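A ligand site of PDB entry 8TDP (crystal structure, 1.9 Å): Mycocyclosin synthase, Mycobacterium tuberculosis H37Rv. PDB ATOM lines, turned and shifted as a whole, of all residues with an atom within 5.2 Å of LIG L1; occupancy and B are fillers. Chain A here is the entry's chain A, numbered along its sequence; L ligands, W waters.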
ATOM      1  N   MET A  61      -7.411  16.494   8.643  1.00  0.00           N
ATOM      2  CA  MET A  61      -6.153  15.781   8.830  1.00  0.00           C
ATOM      3  C   MET A  61      -5.675  15.169   7.518  1.00  0.00           C
ATOM      4  O   MET A  61      -4.497  15.271   7.145  1.00  0.00           O
ATOM      5  CB  MET A  61      -6.304  14.685   9.897  1.00  0.00           C
ATOM      6  CG  MET A  61      -5.295  13.538   9.746  1.00  0.00           C
ATOM      7  SD  MET A  61      -5.380  12.320  11.114  1.00  0.00           S
ATOM      8  CE  MET A  61      -4.823  13.331  12.474  1.00  0.00           C
ATOM      9  N   THR A  76       6.735  10.436   7.026  1.00  0.00           N
ATOM     10  CA  THR A  76       7.503   9.211   7.188  1.00  0.00           C
ATOM     11  C   THR A  76       6.688   7.982   6.842  1.00  0.00           C
ATOM     12  O   THR A  76       7.171   6.862   7.006  1.00  0.00           O
ATOM     13  CB  THR A  76       8.069   9.108   8.615  1.00  0.00           C
ATOM     14  OG1 THR A  76       7.021   8.894   9.566  1.00  0.00           O
ATOM     15  CG2 THR A  76       8.788  10.390   8.999  1.00  0.00           C
ATOM     16  N   VAL A  77       5.463   8.171   6.348  1.00  0.00           N
ATOM     17  CA  VAL A  77       4.590   7.067   5.927  1.00  0.00           C
ATOM     18  C   VAL A  77       4.127   7.378   4.520  1.00  0.00           C
ATOM     19  O   VAL A  77       4.263   8.522   4.051  1.00  0.00           O
ATOM     20  CB  VAL A  77       3.382   6.898   6.897  1.00  0.00           C
ATOM     21  CG1 VAL A  77       3.863   6.494   8.293  1.00  0.00           C
ATOM     22  CG2 VAL A  77       2.573   8.192   6.960  1.00  0.00           C
ATOM     23  N   VAL A  81      -1.583   6.716   4.310  1.00  0.00           N
ATOM     24  CA  VAL A  81      -1.669   6.279   5.704  1.00  0.00           C
ATOM     25  C   VAL A  81      -1.988   7.439   6.649  1.00  0.00           C
ATOM     26  O   VAL A  81      -2.370   7.213   7.806  1.00  0.00           O
ATOM     27  CB  VAL A  81      -0.363   5.536   6.100  1.00  0.00           C
ATOM     28  CG1 VAL A  81      -0.355   5.143   7.596  1.00  0.00           C
ATOM     29  CG2 VAL A  81      -0.218   4.291   5.242  1.00  0.00           C
ATOM     30  N   VAL A  82      -1.870   8.686   6.201  1.00  0.00           N
ATOM     31  CA  VAL A  82      -2.365   9.783   7.024  1.00  0.00           C
ATOM     32  C   VAL A  82      -3.871   9.643   7.244  1.00  0.00           C
ATOM     33  O   VAL A  82      -4.387  10.018   8.304  1.00  0.00           O
ATOM     34  CB  VAL A  82      -1.993  11.128   6.369  1.00  0.00           C
ATOM     35  CG1 VAL A  82      -2.518  12.283   7.168  1.00  0.00           C
ATOM     36  CG2 VAL A  82      -0.469  11.242   6.212  1.00  0.00           C
ATOM     37  N   ASN A  84      -5.353   6.846   7.797  1.00  0.00           N
ATOM     38  CA  ASN A  84      -5.422   5.476   8.290  1.00  0.00           C
ATOM     39  C   ASN A  84      -6.794   5.121   8.876  1.00  0.00           C
ATOM     40  O   ASN A  84      -7.387   4.094   8.517  1.00  0.00           O
ATOM     41  CB  ASN A  84      -4.329   5.266   9.341  1.00  0.00           C
ATOM     42  CG  ASN A  84      -4.074   3.796   9.645  1.00  0.00           C
ATOM     43  OD1 ASN A  84      -4.097   2.957   8.745  1.00  0.00           O
ATOM     44  ND2 ASN A  84      -3.774   3.494  10.902  1.00  0.00           N
ATOM     45  N   ALA A 166      10.910   6.372  12.656  1.00  0.00           N
ATOM     46  CA  ALA A 166       9.535   6.508  12.174  1.00  0.00           C
ATOM     47  C   ALA A 166       8.849   7.750  12.742  1.00  0.00           C
ATOM     48  O   ALA A 166       8.056   8.406  12.057  1.00  0.00           O
ATOM     49  CB  ALA A 166       8.751   5.257  12.546  1.00  0.00           C
ATOM     50  N   PHE A 167       9.120   8.099  14.009  1.00  0.00           N
ATOM     51  CA  PHE A 167       8.432   9.209  14.641  1.00  0.00           C
ATOM     52  C   PHE A 167       9.303  10.439  14.756  1.00  0.00           C
ATOM     53  O   PHE A 167       9.070  11.337  15.566  1.00  0.00           O
ATOM     54  CB  PHE A 167       7.854   8.782  15.982  1.00  0.00           C
ATOM     55  CG  PHE A 167       6.625   7.981  15.816  1.00  0.00           C
ATOM     56  CD1 PHE A 167       6.690   6.600  15.638  1.00  0.00           C
ATOM     57  CD2 PHE A 167       5.391   8.607  15.718  1.00  0.00           C
ATOM     58  CE1 PHE A 167       5.525   5.845  15.429  1.00  0.00           C
ATOM     59  CE2 PHE A 167       4.228   7.865  15.506  1.00  0.00           C
ATOM     60  CZ  PHE A 167       4.308   6.497  15.364  1.00  0.00           C
ATOM     61  N   TRP A 181       9.835   0.877   7.017  1.00  0.00           N
ATOM     62  CA  TRP A 181       8.412   0.705   6.739  1.00  0.00           C
ATOM     63  C   TRP A 181       8.173  -0.524   5.871  1.00  0.00           C
ATOM     64  O   TRP A 181       7.308  -1.359   6.172  1.00  0.00           O
ATOM     65  CB  TRP A 181       7.835   1.942   6.058  1.00  0.00           C
ATOM     66  CG  TRP A 181       6.380   1.807   5.689  1.00  0.00           C
ATOM     67  CD1 TRP A 181       5.866   1.409   4.488  1.00  0.00           C
ATOM     68  CD2 TRP A 181       5.262   2.068   6.543  1.00  0.00           C
ATOM     69  NE1 TRP A 181       4.484   1.424   4.536  1.00  0.00           N
ATOM     70  CE2 TRP A 181       4.087   1.813   5.792  1.00  0.00           C
ATOM     71  CE3 TRP A 181       5.128   2.511   7.872  1.00  0.00           C
ATOM     72  CZ2 TRP A 181       2.800   1.979   6.314  1.00  0.00           C
ATOM     73  CZ3 TRP A 181       3.839   2.663   8.397  1.00  0.00           C
ATOM     74  CH2 TRP A 181       2.706   2.390   7.624  1.00  0.00           C
ATOM     75  N   VAL A 227       1.117  -2.467  11.624  1.00  0.00           N
ATOM     76  CA  VAL A 227       2.287  -1.611  11.760  1.00  0.00           C
ATOM     77  C   VAL A 227       1.905  -0.287  12.433  1.00  0.00           C
ATOM     78  O   VAL A 227       2.555   0.162  13.385  1.00  0.00           O
ATOM     79  CB  VAL A 227       2.960  -1.359  10.395  1.00  0.00           C
ATOM     80  CG1 VAL A 227       4.040  -0.270  10.522  1.00  0.00           C
ATOM     81  CG2 VAL A 227       3.528  -2.666   9.811  1.00  0.00           C
ATOM     82  N   THR A 228       0.835   0.355  11.945  1.00  0.00           N
ATOM     83  CA  THR A 228       0.468   1.670  12.482  1.00  0.00           C
ATOM     84  C   THR A 228       0.037   1.587  13.930  1.00  0.00           C
ATOM     85  O   THR A 228       0.398   2.462  14.746  1.00  0.00           O
ATOM     86  CB  THR A 228      -0.636   2.322  11.641  1.00  0.00           C
ATOM     87  OG1 THR A 228      -1.678   1.366  11.442  1.00  0.00           O
ATOM     88  CG2 THR A 228      -0.091   2.767  10.293  1.00  0.00           C
ATOM     89  N   GLY A 231       3.093   0.974  16.141  1.00  0.00           N
ATOM     90  CA  GLY A 231       3.953   2.143  16.235  1.00  0.00           C
ATOM     91  C   GLY A 231       3.324   3.272  17.039  1.00  0.00           C
ATOM     92  O   GLY A 231       3.939   3.797  17.980  1.00  0.00           O
ATOM     93  N   ALA A 232       2.095   3.675  16.685  1.00  0.00           N
ATOM     94  CA  ALA A 232       1.464   4.773  17.412  1.00  0.00           C
ATOM     95  C   ALA A 232       1.233   4.413  18.881  1.00  0.00           C
ATOM     96  O   ALA A 232       1.443   5.243  19.778  1.00  0.00           O
ATOM     97  CB  ALA A 232       0.153   5.174  16.745  1.00  0.00           C
ATOM     98  N   SER A 236       3.353   6.242  21.910  1.00  0.00           N
ATOM     99  CA  SER A 236       2.514   7.150  22.688  1.00  0.00           C
ATOM    100  C   SER A 236       2.461   6.717  24.154  1.00  0.00           C
ATOM    101  O   SER A 236       2.596   7.560  25.059  1.00  0.00           O
ATOM    102  CB  SER A 236       1.102   7.217  22.096  1.00  0.00           C
ATOM    103  OG  SER A 236       1.127   7.781  20.769  1.00  0.00           O
ATOM    104  N   PHE A 279       3.572  15.216  23.460  1.00  0.00           N
ATOM    105  CA  PHE A 279       3.508  15.606  22.044  1.00  0.00           C
ATOM    106  C   PHE A 279       4.406  16.823  21.807  1.00  0.00           C
ATOM    107  O   PHE A 279       4.224  17.859  22.443  1.00  0.00           O
ATOM    108  CB  PHE A 279       2.069  15.907  21.603  1.00  0.00           C
ATOM    109  CG  PHE A 279       1.330  14.685  21.107  1.00  0.00           C
ATOM    110  CD1 PHE A 279       0.988  13.671  21.996  1.00  0.00           C
ATOM    111  CD2 PHE A 279       0.963  14.564  19.776  1.00  0.00           C
ATOM    112  CE1 PHE A 279       0.302  12.538  21.552  1.00  0.00           C
ATOM    113  CE2 PHE A 279       0.279  13.446  19.329  1.00  0.00           C
ATOM    114  CZ  PHE A 279      -0.046  12.429  20.220  1.00  0.00           C
ATOM    115  N   GLN A 384       8.693  13.574  17.128  1.00  0.00           N
ATOM    116  CA  GLN A 384       7.271  13.841  17.368  1.00  0.00           C
ATOM    117  C   GLN A 384       6.836  13.695  18.826  1.00  0.00           C
ATOM    118  O   GLN A 384       5.710  14.111  19.166  1.00  0.00           O
ATOM    119  CB  GLN A 384       6.402  12.933  16.492  1.00  0.00           C
ATOM    120  CG  GLN A 384       6.499  13.345  15.025  1.00  0.00           C
ATOM    121  CD  GLN A 384       5.817  12.379  14.094  1.00  0.00           C
ATOM    122  OE1 GLN A 384       4.689  11.934  14.339  1.00  0.00           O
ATOM    123  NE2 GLN A 384       6.503  12.024  13.015  1.00  0.00           N
ATOM    124  N   ARG A 385       7.672  13.129  19.696  1.00  0.00           N
ATOM    125  CA  ARG A 385       7.413  13.079  21.122  1.00  0.00           C
ATOM    126  C   ARG A 385       8.578  13.702  21.881  1.00  0.00           C
ATOM    127  O   ARG A 385       9.711  13.731  21.403  1.00  0.00           O
ATOM    128  CB  ARG A 385       7.226  11.646  21.644  1.00  0.00           C
ATOM    129  CG  ARG A 385       6.007  10.900  21.093  1.00  0.00           C
ATOM    130  CD  ARG A 385       4.678  11.513  21.552  1.00  0.00           C
ATOM    131  NE  ARG A 385       3.555  10.748  21.017  1.00  0.00           N
ATOM    132  CZ  ARG A 385       3.087  10.877  19.785  1.00  0.00           C
ATOM    133  NH1 ARG A 385       3.591  11.787  18.942  1.00  0.00           N
ATOM    134  NH2 ARG A 385       2.115  10.067  19.365  1.00  0.00           N
HETATM  135  O1  LIG L   1      -0.348   9.790   9.733  1.00  0.00           O
HETATM  136  C1  LIG L   1      -0.864   8.949  10.447  1.00  0.00           C
HETATM  137  C2  LIG L   1      -2.277   9.155  10.991  1.00  0.00           C
HETATM  138  C3  LIG L   1      -2.343  10.411  11.894  1.00  0.00           C
HETATM  139  C4  LIG L   1      -1.453  10.270  13.114  1.00  0.00           C
HETATM  140  C5  LIG L   1      -0.146  10.785  13.129  1.00  0.00           C
HETATM  141  C6  LIG L   1       0.653  10.643  14.274  1.00  0.00           C
HETATM  142  C7  LIG L   1       0.146   9.989  15.391  1.00  0.00           C
HETATM  143  O2  LIG L   1       0.955   9.867  16.470  1.00  0.00           O
HETATM  144  C8  LIG L   1      -1.144   9.462  15.368  1.00  0.00           C
HETATM  145  C9  LIG L   1      -1.932   9.616  14.250  1.00  0.00           C
HETATM  146  N1  LIG L   1      -2.789   7.959  11.617  1.00  0.00           N
HETATM  147  N2  LIG L   1      -0.224   7.815  10.766  1.00  0.00           N
HETATM  148  C10 LIG L   1      -0.670   6.746  11.629  1.00  0.00           C
HETATM  149  C11 LIG L   1      -2.147   6.829  11.923  1.00  0.00           C
HETATM  150  O3  LIG L   1      -2.670   5.870  12.457  1.00  0.00           O
HETATM  151  C12 LIG L   1       0.137   6.770  12.947  1.00  0.00           C
HETATM  152  C13 LIG L   1       1.540   6.335  12.622  1.00  0.00           C
HETATM  153  C14 LIG L   1       2.507   7.253  12.207  1.00  0.00           C
HETATM  154  C15 LIG L   1       3.795   6.861  11.862  1.00  0.00           C
HETATM  155  C16 LIG L   1       4.134   5.512  11.939  1.00  0.00           C
HETATM  156  O4  LIG L   1       5.367   5.057  11.634  1.00  0.00           O
HETATM  157  C17 LIG L   1       3.185   4.565  12.372  1.00  0.00           C
HETATM  158  C18 LIG L   1       1.896   4.974  12.691  1.00  0.00           C
HETATM  159  C1  LG2 L   2      -4.655   9.450  17.767  1.00  0.00           C
HETATM  160  C2  LG2 L   2      -2.615  10.633  22.035  1.00  0.00           C
HETATM  161  C3  LG2 L   2      -2.317   5.848  22.995  1.00  0.00           C
HETATM  162  C4  LG2 L   2      -3.473   4.783  18.371  1.00  0.00           C
HETATM  163  C5  LG2 L   2      -4.221  10.190  18.858  1.00  0.00           C
HETATM  164  C6  LG2 L   2      -4.338  11.632  19.047  1.00  0.00           C
HETATM  165  C7  LG2 L   2      -3.760  11.966  20.230  1.00  0.00           C
HETATM  166  C8  LG2 L   2      -3.264  10.746  20.829  1.00  0.00           C
HETATM  167  C9  LG2 L   2      -3.649  13.375  20.849  1.00  0.00           C
HETATM  168  C10 LG2 L   2      -5.021  12.608  18.051  1.00  0.00           C
HETATM  169  C11 LG2 L   2      -4.041  13.068  16.971  1.00  0.00           C
HETATM  170  C12 LG2 L   2      -4.716  14.099  16.068  1.00  0.00           C
HETATM  171  O1  LG2 L   2      -5.923  14.394  16.261  1.00  0.00           O
HETATM  172  O2  LG2 L   2      -4.019  14.622  15.135  1.00  0.00           O
HETATM  173  C13 LG2 L   2      -2.375   9.421  22.678  1.00  0.00           C
HETATM  174  C14 LG2 L   2      -1.830   9.266  24.018  1.00  0.00           C
HETATM  175  C15 LG2 L   2      -1.723   7.946  24.263  1.00  0.00           C
HETATM  176  C16 LG2 L   2      -2.216   7.223  23.100  1.00  0.00           C
HETATM  177  C17 LG2 L   2      -1.432  10.474  24.913  1.00  0.00           C
HETATM  178  C18 LG2 L   2      -1.246   7.174  25.507  1.00  0.00           C
HETATM  179  C19 LG2 L   2      -1.171   7.714  26.726  1.00  0.00           C
HETATM  180  C20 LG2 L   2      -2.651   5.145  21.840  1.00  0.00           C
HETATM  181  C21 LG2 L   2      -2.732   3.700  21.732  1.00  0.00           C
HETATM  182  C22 LG2 L   2      -3.070   3.410  20.450  1.00  0.00           C
HETATM  183  C23 LG2 L   2      -3.164   4.658  19.707  1.00  0.00           C
HETATM  184  C24 LG2 L   2      -2.484   2.777  22.952  1.00  0.00           C
HETATM  185  C25 LG2 L   2      -3.290   2.064  19.736  1.00  0.00           C
HETATM  186  C26 LG2 L   2      -2.811   0.937  20.241  1.00  0.00           C
HETATM  187  C27 LG2 L   2      -3.877   5.941  17.760  1.00  0.00           C
HETATM  188  C28 LG2 L   2      -4.287   6.137  16.371  1.00  0.00           C
HETATM  189  C29 LG2 L   2      -4.608   7.431  16.220  1.00  0.00           C
HETATM  190  C30 LG2 L   2      -4.391   8.112  17.491  1.00  0.00           C
HETATM  191  C31 LG2 L   2      -4.332   5.061  15.267  1.00  0.00           C
HETATM  192  C32 LG2 L   2      -5.110   8.107  14.920  1.00  0.00           C
HETATM  193  C33 LG2 L   2      -6.636   8.282  15.092  1.00  0.00           C
HETATM  194  C34 LG2 L   2      -7.308   8.946  13.881  1.00  0.00           C
HETATM  195  O3  LG2 L   2      -8.574   9.012  13.844  1.00  0.00           O
HETATM  196  O4  LG2 L   2      -6.602   9.426  12.959  1.00  0.00           O
HETATM  197  N1  LG2 L   2      -3.556   9.687  19.960  1.00  0.00           N
HETATM  198  N2  LG2 L   2      -2.607   8.155  22.159  1.00  0.00           N
HETATM  199  N3  LG2 L   2      -2.907   5.691  20.599  1.00  0.00           N
HETATM  200  N4  LG2 L   2      -3.959   7.161  18.410  1.00  0.00           N
HETATM  201 FE1  LG2 L   2      -3.465   7.665  20.366  1.00  0.00          FE
HETATM  202  O   HOH W   1       7.483   5.296   9.348  1.00  0.00           O
HETATM  203  O   HOH W   2       6.102   2.504  12.030  1.00  0.00           O
HETATM  204  O   HOH W   3       2.663  12.368  16.145  1.00  0.00           O
HETATM  205  O   HOH W   4       2.159  10.901   9.816  1.00  0.00           O
HETATM  206  O   HOH W   5      -5.793   8.131  10.859  1.00  0.00           O
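Residues that only touch LIG L1: Val 82 (3.4 Å), Val 81 (3.5 Å), Ala 166 (3.5 Å), Phe 167 (3.6 Å), Thr 228 (3.6 Å), Val 77 (3.6 Å) and Met 61 (3.7 Å).
Hydrophobic or aromatic side chains that line LIG L1: Met 61, Val 77, Val 82, Ala 166 and Phe 167.
Of the 17 residues printed, 9 come within 4 Å of LIG L1.
The nearest printed residue that does not touch LIG L1 is Ala 232 (4.1 Å).
Water W3 lies within hydrogen-bond range of OE1 of Gln 384, NH1 of Arg 385 and O2 of LIG L1.
Water W5 lies within hydrogen-bond range of O4 of LG2 L2 (2.6 Å), N1 of LIG L1 (3.1 Å), N of Asn 84 (3.3 Å) and O of Val 82 (3.5 Å).
Water W1 lies within hydrogen-bond range of the backbone carbonyl oxygen (O) of Thr 76 (2.8 Å) and an oxygen (O4) of LIG L1 (3.1 Å).
ND2 of Asn 84 lies within hydrogen-bond range of O3 of LIG L1, 3.0 Å away.
O2 of LIG L1 sits at hydrogen-bond distance from NH2 of Arg 385, 3.1 Å away.
The guanidinium group (NH2) of Arg 385 is in hydrogen-bond range of the side-chain hydroxyl (OG) of Ser 236 (2.9 Å).
The backbone carbonyl oxygen (O) of Phe 167 lies within hydrogen-bond range of the backbone NH (N) of Gln 384, 2.8 Å away.
The backbone carbonyl oxygen (O) of Ala 166 is in hydrogen-bond range of the side-chain hydroxyl (OG1) of Thr 76, 2.7 Å away.
OG1 of Thr 228 sits at hydrogen-bond distance from ND2 of Asn 84 (3.0 Å).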
